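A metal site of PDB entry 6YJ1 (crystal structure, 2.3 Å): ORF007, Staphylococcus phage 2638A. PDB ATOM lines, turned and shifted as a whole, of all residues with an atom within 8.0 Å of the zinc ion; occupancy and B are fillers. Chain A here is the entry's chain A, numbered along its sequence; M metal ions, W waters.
NH1 of Arg 44 lies within salt-bridge range of OD2 of Asp 65 (3.2 Å). The backbone NH (N) of Ser 29 is in hydrogen-bond range of the backbone carbonyl oxygen (O) of Asp 65 (3.1 Å). The backbone carbonyl oxygen (O) of Asp 65 sits at hydrogen-bond distance from the backbone NH (N) of Ser 28, 2.8 Å away. The side-chain amide oxygen (OE1) of Gln 149 lies within hydrogen-bond range of a ring nitrogen (NE2) of His 147, at 3.0 Å. The backbone NH (N) of Gly 108 is in hydrogen-bond range of the backbone carbonyl oxygen (O) of His 147 (2.9 Å). NH1 of Arg 44 is in hydrogen-bond range of ND1 of His 61. ND1 of His 61 lies close to O of Ala 63 (3.3 Å). The side-chain hydroxyl (OH) of Tyr 34 is in hydrogen-bond range of a ring nitrogen (ND1) of His 61 (2.8 Å).
Within 4 Å of the zinc ion: His 61, Asp 65 and His 147.
The zinc ion is bound by water W1 (1.9 Å), OD1 of Asp 65 (2.0 Å), ND1 of His 147 (2.0 Å) and NE2 of His 61 (2.1 Å). The zinc ion has four donor atoms within binding distance. Slightly farther from the zinc ion lies the side-chain carboxylate (OD2) of Asp 65 (2.8 Å).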
ATOM      1  N   SER A  28      29.028  24.073 -28.793  1.00  0.00           N
ATOM      2  CA  SER A  28      28.479  24.860 -29.890  1.00  0.00           C
ATOM      3  C   SER A  28      27.842  26.186 -29.437  1.00  0.00           C
ATOM      4  O   SER A  28      27.842  27.144 -30.215  1.00  0.00           O
ATOM      5  CB  SER A  28      27.435  24.030 -30.634  1.00  0.00           C
ATOM      6  OG  SER A  28      26.730  23.198 -29.743  1.00  0.00           O
ATOM      7  N   SER A  29      27.331  26.261 -28.210  1.00  0.00           N
ATOM      8  CA  SER A  29      26.781  27.531 -27.715  1.00  0.00           C
ATOM      9  C   SER A  29      27.034  27.653 -26.223  1.00  0.00           C
ATOM     10  O   SER A  29      26.698  26.758 -25.439  1.00  0.00           O
ATOM     11  CB  SER A  29      25.287  27.652 -28.018  1.00  0.00           C
ATOM     12  OG  SER A  29      24.818  28.968 -27.722  1.00  0.00           O
ATOM     13  N   TYR A  34      27.915  35.132 -24.742  1.00  0.00           N
ATOM     14  CA  TYR A  34      26.854  36.023 -25.181  1.00  0.00           C
ATOM     15  C   TYR A  34      27.204  37.442 -24.766  1.00  0.00           C
ATOM     16  O   TYR A  34      27.961  37.657 -23.811  1.00  0.00           O
ATOM     17  CB  TYR A  34      25.495  35.594 -24.619  1.00  0.00           C
ATOM     18  CG  TYR A  34      25.110  34.140 -24.909  1.00  0.00           C
ATOM     19  CD1 TYR A  34      25.740  33.386 -25.918  1.00  0.00           C
ATOM     20  CD2 TYR A  34      24.104  33.510 -24.175  1.00  0.00           C
ATOM     21  CE1 TYR A  34      25.391  32.035 -26.155  1.00  0.00           C
ATOM     22  CE2 TYR A  34      23.736  32.171 -24.414  1.00  0.00           C
ATOM     23  CZ  TYR A  34      24.371  31.437 -25.399  1.00  0.00           C
ATOM     24  OH  TYR A  34      23.988  30.129 -25.615  1.00  0.00           O
ATOM     25  N   ARG A  44      20.627  35.159 -25.902  1.00  0.00           N
ATOM     26  CA  ARG A  44      21.284  34.673 -27.101  1.00  0.00           C
ATOM     27  C   ARG A  44      20.601  35.126 -28.369  1.00  0.00           C
ATOM     28  O   ARG A  44      21.275  35.559 -29.301  1.00  0.00           O
ATOM     29  CB  ARG A  44      21.379  33.147 -27.080  1.00  0.00           C
ATOM     30  CG  ARG A  44      22.221  32.661 -28.237  1.00  0.00           C
ATOM     31  CD  ARG A  44      22.297  31.179 -28.272  1.00  0.00           C
ATOM     32  NE  ARG A  44      20.990  30.630 -28.541  1.00  0.00           N
ATOM     33  CZ  ARG A  44      20.757  29.326 -28.659  1.00  0.00           C
ATOM     34  NH1 ARG A  44      21.757  28.448 -28.507  1.00  0.00           N
ATOM     35  NH2 ARG A  44      19.537  28.905 -28.912  1.00  0.00           N
ATOM     36  N   TYR A  46      19.133  33.519 -30.898  1.00  0.00           N
ATOM     37  CA  TYR A  46      19.656  32.805 -32.049  1.00  0.00           C
ATOM     38  C   TYR A  46      18.520  32.558 -33.032  1.00  0.00           C
ATOM     39  O   TYR A  46      17.568  31.825 -32.750  1.00  0.00           O
ATOM     40  CB  TYR A  46      20.311  31.484 -31.646  1.00  0.00           C
ATOM     41  CG  TYR A  46      20.749  30.697 -32.867  1.00  0.00           C
ATOM     42  CD1 TYR A  46      21.169  31.346 -34.021  1.00  0.00           C
ATOM     43  CD2 TYR A  46      20.717  29.302 -32.869  1.00  0.00           C
ATOM     44  CE1 TYR A  46      21.533  30.645 -35.147  1.00  0.00           C
ATOM     45  CE2 TYR A  46      21.112  28.601 -33.987  1.00  0.00           C
ATOM     46  CZ  TYR A  46      21.515  29.269 -35.124  1.00  0.00           C
ATOM     47  OH  TYR A  46      21.891  28.570 -36.241  1.00  0.00           O
ATOM     48  N   TYR A  53      15.131  30.583 -32.729  1.00  0.00           N
ATOM     49  CA  TYR A  53      15.322  29.399 -31.880  1.00  0.00           C
ATOM     50  C   TYR A  53      15.046  29.679 -30.403  1.00  0.00           C
ATOM     51  O   TYR A  53      14.681  28.744 -29.676  1.00  0.00           O
ATOM     52  CB  TYR A  53      16.727  28.828 -32.042  1.00  0.00           C
ATOM     53  CG  TYR A  53      16.904  28.123 -33.359  1.00  0.00           C
ATOM     54  CD1 TYR A  53      17.352  28.815 -34.478  1.00  0.00           C
ATOM     55  CD2 TYR A  53      16.583  26.774 -33.503  1.00  0.00           C
ATOM     56  CE1 TYR A  53      17.514  28.177 -35.710  1.00  0.00           C
ATOM     57  CE2 TYR A  53      16.756  26.138 -34.726  1.00  0.00           C
ATOM     58  CZ  TYR A  53      17.219  26.852 -35.812  1.00  0.00           C
ATOM     59  OH  TYR A  53      17.394  26.223 -37.017  1.00  0.00           O
ATOM     60  N   ASP A  54      15.165  30.906 -29.952  1.00  0.00           N
ATOM     61  CA  ASP A  54      14.897  31.220 -28.554  1.00  0.00           C
ATOM     62  C   ASP A  54      13.587  31.982 -28.378  1.00  0.00           C
ATOM     63  O   ASP A  54      13.427  32.726 -27.401  1.00  0.00           O
ATOM     64  CB  ASP A  54      16.064  31.990 -27.964  1.00  0.00           C
ATOM     65  CG  ASP A  54      17.399  31.409 -28.361  1.00  0.00           C
ATOM     66  OD1 ASP A  54      17.581  30.179 -28.192  1.00  0.00           O
ATOM     67  OD2 ASP A  54      18.261  32.180 -28.819  1.00  0.00           O
ATOM     68  N   TYR A  60      16.163  33.941 -24.600  1.00  0.00           N
ATOM     69  CA  TYR A  60      17.125  33.475 -23.609  1.00  0.00           C
ATOM     70  C   TYR A  60      17.462  32.004 -23.809  1.00  0.00           C
ATOM     71  O   TYR A  60      16.602  31.196 -24.176  1.00  0.00           O
ATOM     72  CB  TYR A  60      16.599  33.729 -22.200  1.00  0.00           C
ATOM     73  CG  TYR A  60      16.818  35.168 -21.819  1.00  0.00           C
ATOM     74  CD1 TYR A  60      15.895  36.152 -22.181  1.00  0.00           C
ATOM     75  CD2 TYR A  60      17.957  35.557 -21.136  1.00  0.00           C
ATOM     76  CE1 TYR A  60      16.105  37.465 -21.848  1.00  0.00           C
ATOM     77  CE2 TYR A  60      18.158  36.866 -20.790  1.00  0.00           C
ATOM     78  CZ  TYR A  60      17.242  37.826 -21.155  1.00  0.00           C
ATOM     79  OH  TYR A  60      17.466  39.158 -20.799  1.00  0.00           O
ATOM     80  N   HIS A  61      18.744  31.668 -23.582  1.00  0.00           N
ATOM     81  CA  HIS A  61      19.216  30.288 -23.737  1.00  0.00           C
ATOM     82  C   HIS A  61      20.107  30.018 -22.531  1.00  0.00           C
ATOM     83  O   HIS A  61      21.330  30.213 -22.560  1.00  0.00           O
ATOM     84  CB  HIS A  61      19.945  30.078 -25.069  1.00  0.00           C
ATOM     85  CG  HIS A  61      20.473  28.677 -25.266  1.00  0.00           C
ATOM     86  ND1 HIS A  61      21.804  28.381 -25.232  1.00  0.00           N
ATOM     87  CD2 HIS A  61      19.825  27.506 -25.469  1.00  0.00           C
ATOM     88  CE1 HIS A  61      21.971  27.089 -25.425  1.00  0.00           C
ATOM     89  NE2 HIS A  61      20.783  26.526 -25.564  1.00  0.00           N
ATOM     90  N   ARG A  62      19.485  29.643 -21.412  1.00  0.00           N
ATOM     91  CA  ARG A  62      20.210  29.560 -20.148  1.00  0.00           C
ATOM     92  C   ARG A  62      20.818  28.174 -19.984  1.00  0.00           C
ATOM     93  O   ARG A  62      20.446  27.418 -19.097  1.00  0.00           O
ATOM     94  CB  ARG A  62      19.293  29.915 -18.986  1.00  0.00           C
ATOM     95  CG  ARG A  62      19.080  31.437 -18.820  1.00  0.00           C
ATOM     96  CD  ARG A  62      18.138  31.759 -17.665  1.00  0.00           C
ATOM     97  NE  ARG A  62      17.670  33.136 -17.714  1.00  0.00           N
ATOM     98  CZ  ARG A  62      16.520  33.519 -18.264  1.00  0.00           C
ATOM     99  NH1 ARG A  62      15.714  32.613 -18.816  1.00  0.00           N
ATOM    100  NH2 ARG A  62      16.196  34.804 -18.265  1.00  0.00           N
ATOM    101  N   ALA A  63      21.738  27.834 -20.882  1.00  0.00           N
ATOM    102  CA  ALA A  63      22.080  26.433 -21.121  1.00  0.00           C
ATOM    103  C   ALA A  63      23.268  26.351 -22.073  1.00  0.00           C
ATOM    104  O   ALA A  63      23.657  27.333 -22.703  1.00  0.00           O
ATOM    105  CB  ALA A  63      20.893  25.656 -21.706  1.00  0.00           C
ATOM    106  N   PHE A  64      23.816  25.147 -22.174  1.00  0.00           N
ATOM    107  CA  PHE A  64      24.924  24.850 -23.058  1.00  0.00           C
ATOM    108  C   PHE A  64      24.454  23.901 -24.150  1.00  0.00           C
ATOM    109  O   PHE A  64      23.860  22.861 -23.861  1.00  0.00           O
ATOM    110  CB  PHE A  64      26.090  24.220 -22.310  1.00  0.00           C
ATOM    111  CG  PHE A  64      27.006  25.204 -21.640  1.00  0.00           C
ATOM    112  CD1 PHE A  64      26.630  25.860 -20.464  1.00  0.00           C
ATOM    113  CD2 PHE A  64      28.267  25.460 -22.169  1.00  0.00           C
ATOM    114  CE1 PHE A  64      27.482  26.770 -19.833  1.00  0.00           C
ATOM    115  CE2 PHE A  64      29.129  26.375 -21.553  1.00  0.00           C
ATOM    116  CZ  PHE A  64      28.722  27.025 -20.371  1.00  0.00           C
ATOM    117  N   ASP A  65      24.741  24.255 -25.403  1.00  0.00           N
ATOM    118  CA  ASP A  65      24.656  23.328 -26.518  1.00  0.00           C
ATOM    119  C   ASP A  65      26.045  22.746 -26.739  1.00  0.00           C
ATOM    120  O   ASP A  65      27.017  23.494 -26.923  1.00  0.00           O
ATOM    121  CB  ASP A  65      24.175  24.036 -27.777  1.00  0.00           C
ATOM    122  CG  ASP A  65      22.751  24.480 -27.672  1.00  0.00           C
ATOM    123  OD1 ASP A  65      22.106  24.023 -26.713  1.00  0.00           O
ATOM    124  OD2 ASP A  65      22.261  25.262 -28.517  1.00  0.00           O
ATOM    125  N   VAL A  66      26.155  21.420 -26.698  1.00  0.00           N
ATOM    126  CA  VAL A  66      27.432  20.743 -26.912  1.00  0.00           C
ATOM    127  C   VAL A  66      27.224  19.641 -27.925  1.00  0.00           C
ATOM    128  O   VAL A  66      26.092  19.194 -28.168  1.00  0.00           O
ATOM    129  CB  VAL A  66      28.010  20.150 -25.612  1.00  0.00           C
ATOM    130  CG1 VAL A  66      28.227  21.223 -24.589  1.00  0.00           C
ATOM    131  CG2 VAL A  66      27.073  19.124 -25.081  1.00  0.00           C
ATOM    132  N   PHE A  91      11.859  20.168 -25.556  1.00  0.00           N
ATOM    133  CA  PHE A  91      13.141  20.112 -26.250  1.00  0.00           C
ATOM    134  C   PHE A  91      13.248  18.862 -27.129  1.00  0.00           C
ATOM    135  O   PHE A  91      14.280  18.190 -27.133  1.00  0.00           O
ATOM    136  CB  PHE A  91      14.301  20.133 -25.261  1.00  0.00           C
ATOM    137  CG  PHE A  91      14.259  21.260 -24.270  1.00  0.00           C
ATOM    138  CD1 PHE A  91      13.760  21.047 -22.979  1.00  0.00           C
ATOM    139  CD2 PHE A  91      14.734  22.529 -24.608  1.00  0.00           C
ATOM    140  CE1 PHE A  91      13.731  22.074 -22.048  1.00  0.00           C
ATOM    141  CE2 PHE A  91      14.697  23.581 -23.697  1.00  0.00           C
ATOM    142  CZ  PHE A  91      14.196  23.349 -22.399  1.00  0.00           C
ATOM    143  N   GLY A 108      18.249  17.698 -23.824  1.00  0.00           N
ATOM    144  CA  GLY A 108      17.267  17.935 -24.856  1.00  0.00           C
ATOM    145  C   GLY A 108      17.740  17.548 -26.231  1.00  0.00           C
ATOM    146  O   GLY A 108      18.952  17.442 -26.457  1.00  0.00           O
ATOM    147  N   HIS A 109      16.785  17.341 -27.154  1.00  0.00           N
ATOM    148  CA  HIS A 109      17.031  17.026 -28.560  1.00  0.00           C
ATOM    149  C   HIS A 109      17.620  15.632 -28.756  1.00  0.00           C
ATOM    150  O   HIS A 109      18.367  15.390 -29.691  1.00  0.00           O
ATOM    151  CB  HIS A 109      17.931  18.079 -29.225  1.00  0.00           C
ATOM    152  CG  HIS A 109      17.534  19.495 -28.932  1.00  0.00           C
ATOM    153  ND1 HIS A 109      16.371  20.067 -29.412  1.00  0.00           N
ATOM    154  CD2 HIS A 109      18.148  20.461 -28.208  1.00  0.00           C
ATOM    155  CE1 HIS A 109      16.289  21.322 -28.990  1.00  0.00           C
ATOM    156  NE2 HIS A 109      17.357  21.578 -28.249  1.00  0.00           N
ATOM    157  N   MET A 142      17.518  21.453 -37.710  1.00  0.00           N
ATOM    158  CA  MET A 142      18.400  21.672 -36.578  1.00  0.00           C
ATOM    159  C   MET A 142      19.629  20.805 -36.737  1.00  0.00           C
ATOM    160  O   MET A 142      19.568  19.703 -37.296  1.00  0.00           O
ATOM    161  CB  MET A 142      17.710  21.357 -35.259  1.00  0.00           C
ATOM    162  CG  MET A 142      18.567  21.668 -34.061  1.00  0.00           C
ATOM    163  SD  MET A 142      17.584  21.340 -32.593  1.00  0.00           S
ATOM    164  CE  MET A 142      16.611  22.844 -32.564  1.00  0.00           C
ATOM    165  N   HIS A 145      22.952  18.020 -31.934  1.00  0.00           N
ATOM    166  CA  HIS A 145      23.694  18.488 -30.770  1.00  0.00           C
ATOM    167  C   HIS A 145      22.907  18.090 -29.526  1.00  0.00           C
ATOM    168  O   HIS A 145      21.754  17.688 -29.600  1.00  0.00           O
ATOM    169  CB  HIS A 145      23.920  20.018 -30.822  1.00  0.00           C
ATOM    170  CG  HIS A 145      22.670  20.819 -30.700  1.00  0.00           C
ATOM    171  ND1 HIS A 145      21.841  21.094 -31.765  1.00  0.00           N
ATOM    172  CD2 HIS A 145      22.074  21.385 -29.613  1.00  0.00           C
ATOM    173  CE1 HIS A 145      20.804  21.795 -31.352  1.00  0.00           C
ATOM    174  NE2 HIS A 145      20.919  21.993 -30.054  1.00  0.00           N
ATOM    175  N   LEU A 146      23.581  18.161 -28.377  1.00  0.00           N
ATOM    176  CA  LEU A 146      22.930  18.035 -27.090  1.00  0.00           C
ATOM    177  C   LEU A 146      22.746  19.421 -26.490  1.00  0.00           C
ATOM    178  O   LEU A 146      23.702  20.210 -26.429  1.00  0.00           O
ATOM    179  CB  LEU A 146      23.732  17.156 -26.119  1.00  0.00           C
ATOM    180  CG  LEU A 146      23.289  17.308 -24.649  1.00  0.00           C
ATOM    181  CD1 LEU A 146      22.015  16.524 -24.404  1.00  0.00           C
ATOM    182  CD2 LEU A 146      24.364  16.926 -23.638  1.00  0.00           C
ATOM    183  N   HIS A 147      21.511  19.735 -26.091  1.00  0.00           N
ATOM    184  CA  HIS A 147      21.196  20.895 -25.272  1.00  0.00           C
ATOM    185  C   HIS A 147      21.170  20.461 -23.806  1.00  0.00           C
ATOM    186  O   HIS A 147      20.389  19.585 -23.437  1.00  0.00           O
ATOM    187  CB  HIS A 147      19.859  21.489 -25.706  1.00  0.00           C
ATOM    188  CG  HIS A 147      19.295  22.525 -24.789  1.00  0.00           C
ATOM    189  ND1 HIS A 147      19.295  23.864 -25.107  1.00  0.00           N
ATOM    190  CD2 HIS A 147      18.648  22.423 -23.608  1.00  0.00           C
ATOM    191  CE1 HIS A 147      18.694  24.547 -24.139  1.00  0.00           C
ATOM    192  NE2 HIS A 147      18.292  23.688 -23.220  1.00  0.00           N
ATOM    193  N   LEU A 148      22.013  21.077 -22.990  1.00  0.00           N
ATOM    194  CA  LEU A 148      22.147  20.751 -21.573  1.00  0.00           C
ATOM    195  C   LEU A 148      21.840  21.997 -20.776  1.00  0.00           C
ATOM    196  O   LEU A 148      22.463  23.042 -20.964  1.00  0.00           O
ATOM    197  CB  LEU A 148      23.558  20.248 -21.246  1.00  0.00           C
ATOM    198  CG  LEU A 148      23.670  19.597 -19.867  1.00  0.00           C
ATOM    199  CD1 LEU A 148      22.883  18.289 -19.840  1.00  0.00           C
ATOM    200  CD2 LEU A 148      25.129  19.352 -19.448  1.00  0.00           C
ATOM    201  N   GLN A 149      20.857  21.894 -19.898  1.00  0.00           N
ATOM    202  CA  GLN A 149      20.362  23.017 -19.129  1.00  0.00           C
ATOM    203  C   GLN A 149      20.157  22.551 -17.704  1.00  0.00           C
ATOM    204  O   GLN A 149      19.758  21.405 -17.474  1.00  0.00           O
ATOM    205  CB  GLN A 149      19.055  23.535 -19.700  1.00  0.00           C
ATOM    206  CG  GLN A 149      18.475  24.747 -18.997  1.00  0.00           C
ATOM    207  CD  GLN A 149      17.215  25.235 -19.691  1.00  0.00           C
ATOM    208  OE1 GLN A 149      17.070  25.078 -20.915  1.00  0.00           O
ATOM    209  NE2 GLN A 149      16.283  25.815 -18.924  1.00  0.00           N
HETATM  210 ZN    ZN M   1      20.299  24.787 -26.563  1.00  0.00          ZN
HETATM  211  O   HOH W   1      19.472  25.095 -28.296  1.00  0.00           O
